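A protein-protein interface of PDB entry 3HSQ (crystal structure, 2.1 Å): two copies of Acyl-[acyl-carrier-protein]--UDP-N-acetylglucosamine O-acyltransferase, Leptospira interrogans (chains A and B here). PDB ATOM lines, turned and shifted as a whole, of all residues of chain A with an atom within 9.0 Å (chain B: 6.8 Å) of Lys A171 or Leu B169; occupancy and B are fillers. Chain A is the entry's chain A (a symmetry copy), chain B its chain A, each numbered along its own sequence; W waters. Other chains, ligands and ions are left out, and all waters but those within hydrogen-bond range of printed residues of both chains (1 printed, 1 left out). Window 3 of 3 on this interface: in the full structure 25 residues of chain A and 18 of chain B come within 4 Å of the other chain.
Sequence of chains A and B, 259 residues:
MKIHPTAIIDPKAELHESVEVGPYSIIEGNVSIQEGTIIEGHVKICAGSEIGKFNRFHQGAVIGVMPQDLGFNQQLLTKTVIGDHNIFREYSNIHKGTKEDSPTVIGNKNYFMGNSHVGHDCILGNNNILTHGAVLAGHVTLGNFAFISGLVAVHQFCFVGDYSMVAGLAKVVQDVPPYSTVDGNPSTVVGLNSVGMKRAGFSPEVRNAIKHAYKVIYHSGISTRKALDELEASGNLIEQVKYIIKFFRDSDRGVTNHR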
ATOM      1  N   GLY A 150       9.334  33.738  -4.379  1.00  0.00           N
ATOM      2  CA  GLY A 150       9.979  32.423  -4.448  1.00  0.00           C
ATOM      3  C   GLY A 150       8.916  31.342  -4.403  1.00  0.00           C
ATOM      4  O   GLY A 150       7.772  31.617  -4.047  1.00  0.00           O
ATOM      5  N   LEU A 151       9.288  30.117  -4.775  1.00  0.00           N
ATOM      6  CA  LEU A 151       8.359  28.970  -4.808  1.00  0.00           C
ATOM      7  C   LEU A 151       7.162  29.197  -5.747  1.00  0.00           C
ATOM      8  O   LEU A 151       6.040  28.764  -5.481  1.00  0.00           O
ATOM      9  CB  LEU A 151       7.915  28.541  -3.382  1.00  0.00           C
ATOM     10  CG  LEU A 151       8.982  28.542  -2.270  1.00  0.00           C
ATOM     11  CD1 LEU A 151       8.384  28.313  -0.899  1.00  0.00           C
ATOM     12  CD2 LEU A 151      10.129  27.525  -2.550  1.00  0.00           C
ATOM     13  N   VAL A 152       7.419  29.878  -6.856  1.00  0.00           N
ATOM     14  CA  VAL A 152       6.410  30.079  -7.893  1.00  0.00           C
ATOM     15  C   VAL A 152       6.844  29.446  -9.223  1.00  0.00           C
ATOM     16  O   VAL A 152       7.972  29.656  -9.688  1.00  0.00           O
ATOM     17  CB  VAL A 152       6.106  31.583  -8.128  1.00  0.00           C
ATOM     18  CG1 VAL A 152       5.062  31.761  -9.243  1.00  0.00           C
ATOM     19  CG2 VAL A 152       5.626  32.239  -6.841  1.00  0.00           C
ATOM     20  N   ALA A 153       5.938  28.677  -9.819  1.00  0.00           N
ATOM     21  CA  ALA A 153       6.092  28.170 -11.178  1.00  0.00           C
ATOM     22  C   ALA A 153       5.155  28.938 -12.093  1.00  0.00           C
ATOM     23  O   ALA A 153       3.944  28.982 -11.860  1.00  0.00           O
ATOM     24  CB  ALA A 153       5.779  26.677 -11.235  1.00  0.00           C
ATOM     25  N   VAL A 154       5.723  29.575 -13.112  1.00  0.00           N
ATOM     26  CA  VAL A 154       4.923  30.259 -14.128  1.00  0.00           C
ATOM     27  C   VAL A 154       5.044  29.491 -15.437  1.00  0.00           C
ATOM     28  O   VAL A 154       6.144  29.168 -15.870  1.00  0.00           O
ATOM     29  CB  VAL A 154       5.370  31.735 -14.338  1.00  0.00           C
ATOM     30  CG1 VAL A 154       4.487  32.411 -15.392  1.00  0.00           C
ATOM     31  CG2 VAL A 154       5.320  32.521 -12.996  1.00  0.00           C
ATOM     32  N   HIS A 155       3.904  29.186 -16.046  1.00  0.00           N
ATOM     33  CA  HIS A 155       3.867  28.463 -17.309  1.00  0.00           C
ATOM     34  C   HIS A 155       4.469  29.323 -18.417  1.00  0.00           C
ATOM     35  O   HIS A 155       4.260  30.548 -18.464  1.00  0.00           O
ATOM     36  CB  HIS A 155       2.419  28.076 -17.651  1.00  0.00           C
ATOM     37  CG  HIS A 155       2.296  26.980 -18.668  1.00  0.00           C
ATOM     38  ND1 HIS A 155       2.573  27.168 -20.007  1.00  0.00           N
ATOM     39  CD2 HIS A 155       1.889  25.696 -18.545  1.00  0.00           C
ATOM     40  CE1 HIS A 155       2.360  26.040 -20.660  1.00  0.00           C
ATOM     41  NE2 HIS A 155       1.941  25.132 -19.798  1.00  0.00           N
ATOM     42  N   CYS A 158       3.066  32.880 -20.466  1.00  0.00           N
ATOM     43  CA  CYS A 158       2.186  33.674 -19.618  1.00  0.00           C
ATOM     44  C   CYS A 158       2.658  35.127 -19.580  1.00  0.00           C
ATOM     45  O   CYS A 158       3.852  35.415 -19.695  1.00  0.00           O
ATOM     46  CB  CYS A 158       2.111  33.092 -18.195  1.00  0.00           C
ATOM     47  SG  CYS A 158       1.105  31.595 -18.010  1.00  0.00           S
ATOM     48  N   VAL A 166       2.582  37.735  -7.587  1.00  0.00           N
ATOM     49  CA  VAL A 166       2.382  36.300  -7.440  1.00  0.00           C
ATOM     50  C   VAL A 166       2.998  35.863  -6.113  1.00  0.00           C
ATOM     51  O   VAL A 166       4.202  35.952  -5.927  1.00  0.00           O
ATOM     52  CB  VAL A 166       2.982  35.486  -8.599  1.00  0.00           C
ATOM     53  CG1 VAL A 166       2.578  34.024  -8.445  1.00  0.00           C
ATOM     54  CG2 VAL A 166       2.507  36.038  -9.947  1.00  0.00           C
ATOM     55  N   ALA A 167       2.144  35.424  -5.195  1.00  0.00           N
ATOM     56  CA  ALA A 167       2.554  34.991  -3.863  1.00  0.00           C
ATOM     57  C   ALA A 167       3.207  33.598  -3.905  1.00  0.00           C
ATOM     58  O   ALA A 167       3.017  32.849  -4.860  1.00  0.00           O
ATOM     59  CB  ALA A 167       1.346  35.011  -2.910  1.00  0.00           C
ATOM     60  N   GLY A 168       3.974  33.275  -2.863  1.00  0.00           N
ATOM     61  CA  GLY A 168       4.736  32.021  -2.774  1.00  0.00           C
ATOM     62  C   GLY A 168       3.875  30.775  -2.755  1.00  0.00           C
ATOM     63  O   GLY A 168       2.737  30.815  -2.287  1.00  0.00           O
ATOM     64  N   LEU A 169       4.415  29.669  -3.265  1.00  0.00           N
ATOM     65  CA  LEU A 169       3.692  28.373  -3.381  1.00  0.00           C
ATOM     66  C   LEU A 169       2.514  28.420  -4.382  1.00  0.00           C
ATOM     67  O   LEU A 169       1.453  27.824  -4.158  1.00  0.00           O
ATOM     68  CB  LEU A 169       3.286  27.809  -1.992  1.00  0.00           C
ATOM     69  CG  LEU A 169       4.470  27.440  -1.076  1.00  0.00           C
ATOM     70  CD1 LEU A 169       4.059  27.216   0.365  1.00  0.00           C
ATOM     71  CD2 LEU A 169       5.199  26.202  -1.620  1.00  0.00           C
ATOM     72  N   ALA A 170       2.723  29.120  -5.496  1.00  0.00           N
ATOM     73  CA  ALA A 170       1.700  29.283  -6.529  1.00  0.00           C
ATOM     74  C   ALA A 170       2.137  28.692  -7.862  1.00  0.00           C
ATOM     75  O   ALA A 170       3.306  28.786  -8.251  1.00  0.00           O
ATOM     76  CB  ALA A 170       1.339  30.759  -6.703  1.00  0.00           C
ATOM     77  N   LYS A 171       1.179  28.077  -8.546  1.00  0.00           N
ATOM     78  CA  LYS A 171       1.375  27.591  -9.909  1.00  0.00           C
ATOM     79  C   LYS A 171       0.536  28.403 -10.904  1.00  0.00           C
ATOM     80  O   LYS A 171      -0.683  28.305 -10.938  1.00  0.00           O
ATOM     81  CB  LYS A 171       1.030  26.116 -10.002  1.00  0.00           C
ATOM     82  CG  LYS A 171       1.382  25.487 -11.339  1.00  0.00           C
ATOM     83  CD  LYS A 171       1.108  24.008 -11.314  1.00  0.00           C
ATOM     84  CE  LYS A 171       2.087  23.267 -10.406  1.00  0.00           C
ATOM     85  NZ  LYS A 171       2.045  21.789 -10.656  1.00  0.00           N
ATOM     86  N   VAL A 172       1.220  29.204 -11.703  1.00  0.00           N
ATOM     87  CA  VAL A 172       0.587  30.106 -12.651  1.00  0.00           C
ATOM     88  C   VAL A 172       0.473  29.414 -14.013  1.00  0.00           C
ATOM     89  O   VAL A 172       1.481  28.985 -14.570  1.00  0.00           O
ATOM     90  CB  VAL A 172       1.403  31.420 -12.766  1.00  0.00           C
ATOM     91  CG1 VAL A 172       0.926  32.276 -13.938  1.00  0.00           C
ATOM     92  CG2 VAL A 172       1.322  32.216 -11.455  1.00  0.00           C
ATOM     93  N   VAL A 173      -0.747  29.309 -14.543  1.00  0.00           N
ATOM     94  CA  VAL A 173      -0.973  28.641 -15.842  1.00  0.00           C
ATOM     95  C   VAL A 173      -1.584  29.535 -16.930  1.00  0.00           C
ATOM     96  O   VAL A 173      -1.469  29.237 -18.120  1.00  0.00           O
ATOM     97  CB  VAL A 173      -1.790  27.300 -15.707  1.00  0.00           C
ATOM     98  CG1 VAL A 173      -1.051  26.301 -14.834  1.00  0.00           C
ATOM     99  CG2 VAL A 173      -3.186  27.549 -15.158  1.00  0.00           C
ATOM    100  N   GLN A 174      -2.249  30.609 -16.511  1.00  0.00           N
ATOM    101  CA  GLN A 174      -2.812  31.609 -17.420  1.00  0.00           C
ATOM    102  C   GLN A 174      -2.299  32.990 -16.999  1.00  0.00           C
ATOM    103  O   GLN A 174      -1.554  33.095 -16.021  1.00  0.00           O
ATOM    104  CB  GLN A 174      -4.344  31.534 -17.411  1.00  0.00           C
ATOM    105  CG  GLN A 174      -4.899  30.339 -18.184  1.00  0.00           C
ATOM    106  CD  GLN A 174      -6.416  30.260 -18.151  1.00  0.00           C
ATOM    107  OE1 GLN A 174      -7.018  30.077 -17.089  1.00  0.00           O
ATOM    108  NE2 GLN A 174      -7.045  30.379 -19.324  1.00  0.00           N
ATOM    109  N   VAL A 176      -1.577  36.704 -15.498  1.00  0.00           N
ATOM    110  CA  VAL A 176      -1.813  37.400 -14.236  1.00  0.00           C
ATOM    111  C   VAL A 176      -2.213  38.853 -14.553  1.00  0.00           C
ATOM    112  O   VAL A 176      -1.404  39.626 -15.058  1.00  0.00           O
ATOM    113  CB  VAL A 176      -0.581  37.341 -13.294  1.00  0.00           C
ATOM    114  CG1 VAL A 176      -0.842  38.117 -11.997  1.00  0.00           C
ATOM    115  CG2 VAL A 176      -0.196  35.886 -12.986  1.00  0.00           C
ATOM    116  N   VAL A 182      -2.180  37.119  -7.185  1.00  0.00           N
ATOM    117  CA  VAL A 182      -2.517  35.749  -7.514  1.00  0.00           C
ATOM    118  C   VAL A 182      -1.856  34.826  -6.494  1.00  0.00           C
ATOM    119  O   VAL A 182      -0.717  35.057  -6.078  1.00  0.00           O
ATOM    120  CB  VAL A 182      -2.088  35.399  -8.969  1.00  0.00           C
ATOM    121  CG1 VAL A 182      -1.947  33.912  -9.152  1.00  0.00           C
ATOM    122  CG2 VAL A 182      -3.099  35.968  -9.979  1.00  0.00           C
ATOM    123  N   ASP A 183      -2.587  33.792  -6.082  1.00  0.00           N
ATOM    124  CA  ASP A 183      -2.119  32.907  -5.038  1.00  0.00           C
ATOM    125  C   ASP A 183      -2.651  31.484  -5.217  1.00  0.00           C
ATOM    126  O   ASP A 183      -3.667  31.270  -5.875  1.00  0.00           O
ATOM    127  CB  ASP A 183      -2.523  33.465  -3.670  1.00  0.00           C
ATOM    128  CG  ASP A 183      -1.795  32.799  -2.526  1.00  0.00           C
ATOM    129  OD1 ASP A 183      -0.775  32.117  -2.760  1.00  0.00           O
ATOM    130  OD2 ASP A 183      -2.236  32.973  -1.382  1.00  0.00           O
ATOM    131  N   GLY A 184      -1.943  30.525  -4.638  1.00  0.00           N
ATOM    132  CA  GLY A 184      -2.421  29.148  -4.553  1.00  0.00           C
ATOM    133  C   GLY A 184      -2.079  28.236  -5.711  1.00  0.00           C
ATOM    134  O   GLY A 184      -1.544  28.662  -6.729  1.00  0.00           O
ATOM    135  N   ASN A 185      -2.404  26.963  -5.530  1.00  0.00           N
ATOM    136  CA  ASN A 185      -2.223  25.944  -6.544  1.00  0.00           C
ATOM    137  C   ASN A 185      -3.428  25.008  -6.503  1.00  0.00           C
ATOM    138  O   ASN A 185      -3.615  24.297  -5.509  1.00  0.00           O
ATOM    139  CB  ASN A 185      -0.918  25.178  -6.302  1.00  0.00           C
ATOM    140  CG  ASN A 185      -0.738  23.993  -7.235  1.00  0.00           C
ATOM    141  OD1 ASN A 185      -1.144  24.021  -8.406  1.00  0.00           O
ATOM    142  ND2 ASN A 185      -0.107  22.937  -6.718  1.00  0.00           N
ATOM    143  N   PRO A 186      -4.259  25.025  -7.564  1.00  0.00           N
ATOM    144  CA  PRO A 186      -4.125  25.895  -8.745  1.00  0.00           C
ATOM    145  C   PRO A 186      -4.426  27.356  -8.404  1.00  0.00           C
ATOM    146  O   PRO A 186      -5.227  27.633  -7.510  1.00  0.00           O
ATOM    147  CB  PRO A 186      -5.156  25.338  -9.730  1.00  0.00           C
ATOM    148  CG  PRO A 186      -6.137  24.588  -8.905  1.00  0.00           C
ATOM    149  CD  PRO A 186      -5.445  24.152  -7.638  1.00  0.00           C
ATOM    150  N   SER A 187      -3.779  28.280  -9.103  1.00  0.00           N
ATOM    151  CA  SER A 187      -3.788  29.671  -8.669  1.00  0.00           C
ATOM    152  C   SER A 187      -5.027  30.408  -9.127  1.00  0.00           C
ATOM    153  O   SER A 187      -5.648  30.031 -10.123  1.00  0.00           O
ATOM    154  CB  SER A 187      -2.505  30.397  -9.090  1.00  0.00           C
ATOM    155  OG  SER A 187      -2.524  30.774 -10.449  1.00  0.00           O
ATOM    156  N   THR A 188      -5.387  31.442  -8.368  1.00  0.00           N
ATOM    157  CA  THR A 188      -6.499  32.321  -8.698  1.00  0.00           C
ATOM    158  C   THR A 188      -6.133  33.741  -8.340  1.00  0.00           C
ATOM    159  O   THR A 188      -5.243  33.964  -7.522  1.00  0.00           O
ATOM    160  CB  THR A 188      -7.780  31.971  -7.900  1.00  0.00           C
ATOM    161  OG1 THR A 188      -7.479  31.915  -6.503  1.00  0.00           O
ATOM    162  CG2 THR A 188      -8.384  30.640  -8.346  1.00  0.00           C
ATOM    163  N   THR A 256      -6.110  34.261 -15.684  1.00  0.00           N
ATOM    164  CA  THR A 256      -6.436  33.547 -14.444  1.00  0.00           C
ATOM    165  C   THR A 256      -7.783  33.991 -13.851  1.00  0.00           C
ATOM    166  O   THR A 256      -8.074  35.177 -13.767  1.00  0.00           O
ATOM    167  CB  THR A 256      -5.315  33.701 -13.385  1.00  0.00           C
ATOM    168  OG1 THR A 256      -4.059  33.312 -13.955  1.00  0.00           O
ATOM    169  CG2 THR A 256      -5.595  32.832 -12.169  1.00  0.00           C
ATOM    170  N   SER B 149      10.556  18.055 -11.845  1.00  0.00           N
ATOM    171  CA  SER B 149      10.330  19.498 -11.851  1.00  0.00           C
ATOM    172  C   SER B 149      10.912  20.152 -10.606  1.00  0.00           C
ATOM    173  O   SER B 149      11.184  19.477  -9.602  1.00  0.00           O
ATOM    174  CB  SER B 149       8.835  19.811 -11.968  1.00  0.00           C
ATOM    175  OG  SER B 149       8.278  19.207 -13.129  1.00  0.00           O
ATOM    176  N   GLY B 150      11.128  21.464 -10.685  1.00  0.00           N
ATOM    177  CA  GLY B 150      11.488  22.270  -9.516  1.00  0.00           C
ATOM    178  C   GLY B 150      10.336  22.264  -8.530  1.00  0.00           C
ATOM    179  O   GLY B 150       9.222  21.886  -8.886  1.00  0.00           O
ATOM    180  N   LEU B 151      10.605  22.669  -7.288  1.00  0.00           N
ATOM    181  CA  LEU B 151       9.592  22.692  -6.214  1.00  0.00           C
ATOM    182  C   LEU B 151       8.987  21.307  -5.931  1.00  0.00           C
ATOM    183  O   LEU B 151       7.803  21.171  -5.619  1.00  0.00           O
ATOM    184  CB  LEU B 151       8.503  23.770  -6.466  1.00  0.00           C
ATOM    185  CG  LEU B 151       8.959  25.133  -7.024  1.00  0.00           C
ATOM    186  CD1 LEU B 151       7.793  26.011  -7.422  1.00  0.00           C
ATOM    187  CD2 LEU B 151       9.908  25.885  -6.044  1.00  0.00           C
ATOM    188  N   VAL B 152       9.820  20.281  -6.038  1.00  0.00           N
ATOM    189  CA  VAL B 152       9.418  18.918  -5.697  1.00  0.00           C
ATOM    190  C   VAL B 152      10.266  18.360  -4.545  1.00  0.00           C
ATOM    191  O   VAL B 152      11.500  18.440  -4.568  1.00  0.00           O
ATOM    192  CB  VAL B 152       9.525  17.957  -6.912  1.00  0.00           C
ATOM    193  CG1 VAL B 152       9.122  16.527  -6.512  1.00  0.00           C
ATOM    194  CG2 VAL B 152       8.660  18.450  -8.062  1.00  0.00           C
ATOM    195  N   ALA B 153       9.587  17.798  -3.549  1.00  0.00           N
ATOM    196  CA  ALA B 153      10.223  17.033  -2.483  1.00  0.00           C
ATOM    197  C   ALA B 153       9.934  15.558  -2.704  1.00  0.00           C
ATOM    198  O   ALA B 153       8.773  15.152  -2.796  1.00  0.00           O
ATOM    199  CB  ALA B 153       9.701  17.473  -1.118  1.00  0.00           C
ATOM    200  N   ALA B 167       5.448  16.742 -11.489  1.00  0.00           N
ATOM    201  CA  ALA B 167       5.151  18.149 -11.733  1.00  0.00           C
ATOM    202  C   ALA B 167       5.493  19.014 -10.507  1.00  0.00           C
ATOM    203  O   ALA B 167       5.606  18.502  -9.395  1.00  0.00           O
ATOM    204  CB  ALA B 167       3.675  18.313 -12.134  1.00  0.00           C
ATOM    205  N   GLY B 168       5.657  20.318 -10.731  1.00  0.00           N
ATOM    206  CA  GLY B 168       6.063  21.275  -9.693  1.00  0.00           C
ATOM    207  C   GLY B 168       5.070  21.414  -8.558  1.00  0.00           C
ATOM    208  O   GLY B 168       3.870  21.225  -8.758  1.00  0.00           O
ATOM    209  N   LEU B 169       5.569  21.741  -7.366  1.00  0.00           N
ATOM    210  CA  LEU B 169       4.747  21.860  -6.130  1.00  0.00           C
ATOM    211  C   LEU B 169       4.153  20.512  -5.661  1.00  0.00           C
ATOM    212  O   LEU B 169       3.012  20.440  -5.188  1.00  0.00           O
ATOM    213  CB  LEU B 169       3.683  22.984  -6.249  1.00  0.00           C
ATOM    214  CG  LEU B 169       4.260  24.407  -6.393  1.00  0.00           C
ATOM    215  CD1 LEU B 169       3.230  25.424  -6.837  1.00  0.00           C
ATOM    216  CD2 LEU B 169       4.917  24.852  -5.077  1.00  0.00           C
ATOM    217  N   ALA B 170       4.950  19.449  -5.781  1.00  0.00           N
ATOM    218  CA  ALA B 170       4.527  18.101  -5.407  1.00  0.00           C
ATOM    219  C   ALA B 170       5.386  17.524  -4.291  1.00  0.00           C
ATOM    220  O   ALA B 170       6.603  17.731  -4.247  1.00  0.00           O
ATOM    221  CB  ALA B 170       4.550  17.172  -6.621  1.00  0.00           C
ATOM    222  N   LYS B 171       4.727  16.803  -3.389  1.00  0.00           N
ATOM    223  CA  LYS B 171       5.406  16.046  -2.341  1.00  0.00           C
ATOM    224  C   LYS B 171       5.247  14.537  -2.569  1.00  0.00           C
ATOM    225  O   LYS B 171       4.169  13.980  -2.412  1.00  0.00           O
ATOM    226  CB  LYS B 171       4.875  16.437  -0.975  1.00  0.00           C
ATOM    227  CG  LYS B 171       5.655  15.833   0.181  1.00  0.00           C
ATOM    228  CD  LYS B 171       5.134  16.349   1.495  1.00  0.00           C
ATOM    229  CE  LYS B 171       5.468  17.827   1.694  1.00  0.00           C
ATOM    230  NZ  LYS B 171       5.273  18.239   3.121  1.00  0.00           N
ATOM    231  N   ASP B 183       1.367  14.524  -9.425  1.00  0.00           N
ATOM    232  CA  ASP B 183       1.165  15.928  -9.138  1.00  0.00           C
ATOM    233  C   ASP B 183       0.517  16.141  -7.770  1.00  0.00           C
ATOM    234  O   ASP B 183      -0.132  15.246  -7.233  1.00  0.00           O
ATOM    235  CB  ASP B 183       0.314  16.562 -10.242  1.00  0.00           C
ATOM    236  CG  ASP B 183       0.337  18.072 -10.208  1.00  0.00           C
ATOM    237  OD1 ASP B 183       1.215  18.658  -9.540  1.00  0.00           O
ATOM    238  OD2 ASP B 183      -0.518  18.678 -10.868  1.00  0.00           O
ATOM    239  N   GLY B 184       0.716  17.329  -7.214  1.00  0.00           N
ATOM    240  CA  GLY B 184       0.007  17.753  -6.010  1.00  0.00           C
ATOM    241  C   GLY B 184       0.649  17.404  -4.686  1.00  0.00           C
ATOM    242  O   GLY B 184       1.641  16.685  -4.620  1.00  0.00           O
ATOM    243  N   ASN B 185       0.053  17.929  -3.624  1.00  0.00           N
ATOM    244  CA  ASN B 185       0.470  17.660  -2.263  1.00  0.00           C
ATOM    245  C   ASN B 185      -0.780  17.523  -1.397  1.00  0.00           C
ATOM    246  O   ASN B 185      -1.506  18.506  -1.213  1.00  0.00           O
ATOM    247  CB  ASN B 185       1.377  18.785  -1.750  1.00  0.00           C
ATOM    248  CG  ASN B 185       1.727  18.649  -0.280  1.00  0.00           C
ATOM    249  OD1 ASN B 185       1.884  17.539   0.250  1.00  0.00           O
ATOM    250  ND2 ASN B 185       1.867  19.792   0.392  1.00  0.00           N
HETATM  251  O   HOH W   1       1.096  21.772  -4.293  1.00  0.00           O
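Among the printed residues, pairs that only touch across the chains: Ala A170 with Leu B169 (3.6 Å), Leu A151 with Leu B151 (3.7 Å), Leu A169 with Leu B169 (3.7 Å), Lys A171 with Leu B169 (3.8 Å), Asn A185 with Leu B169 (3.8 Å) and Val A152 with Leu B151 (3.9 Å).
O of Gly B168 sits at hydrogen-bond distance from NZ of Lys A171, 2.7 Å away.
The side-chain carboxylate of Asp B183 lies within salt-bridge range of the side-chain amino group of Lys A171, at 3.4 Å.
Ala A170 touches Leu B169, but with the chains exchanged Leu A169 does not touch Ala B170 (7.9 Å).
Lys A171 touches Leu B169, but with the chains exchanged Leu A169 does not touch Lys B171 (9.0 Å).
Lys A171 touches Asp B183, but with the chains exchanged Asp A183 does not touch Lys B171 (16.2 Å).
Asn A185 touches Leu B169, but with the chains exchanged Leu A169 does not touch Asn B185 (7.5 Å).
Water W1 bridges the backbone carbonyl oxygen (O) of Leu B169 (2.5 Å) and the side-chain amide nitrogen (ND2) of Asn A185 (2.9 Å).
Of the printed residues of chain B, Leu A151 touches Leu B151.
Of the printed residues of chain B, Leu A169 touches Leu B169.
Printed residues of chain B within 4 Å of Ala A170: Leu B169.
Lys A171 touches just these residues of chain B: Gly B168 (2.7 Å), Leu B169 (3.8 Å) and Asp B183 (3.4 Å).
Gly B168 touches one residue of chain A.
No residue of chain A comes within 4 Å of Ala B170.
Lys B171 touches none of the printed residues of chain A.
No residue of chain A comes within 4 Å of Gly B184.
Printed residues of chain B that touch a printed residue of chain A: Leu B151, Gly B168, Leu B169 and Asp B183.
Hydrophobic or aromatic side chains of chain B that line the printed part of chain A: Leu B151 and Leu B169.
Of the 25 printed residues of chain A, 6 touch a printed residue of chain B.
Along chain A the printed residues that touch a printed residue of chain B span positions 151 to 185.
Among the printed residues, 8 pairs touch across the chains.
Among the printed residues, Asp or Glu carboxylates within 4 Å of a Lys or Arg side-chain nitrogen of the other chain: Lys A171 with Asp B183 (3.4 Å).
O of Leu B151 sits at hydrogen-bond distance from N of Leu B169, at 2.9 Å.
O of Leu B151 lies within hydrogen-bond range of N of Ala B170.
The backbone carbonyl oxygen of Leu A151 sits at hydrogen-bond distance from the backbone NH of Leu A169 (2.9 Å).
The backbone carbonyl oxygen (O) of Ala A170 sits at hydrogen-bond distance from the backbone NH (N) of Ala A153, 3.1 Å away.
The backbone NH (N) of Lys A171 sits at hydrogen-bond distance from the backbone carbonyl oxygen (O) of Gly A184 (3.3 Å).
OG of Ser A187 is in hydrogen-bond range of O of Lys A171, at 3.1 Å.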
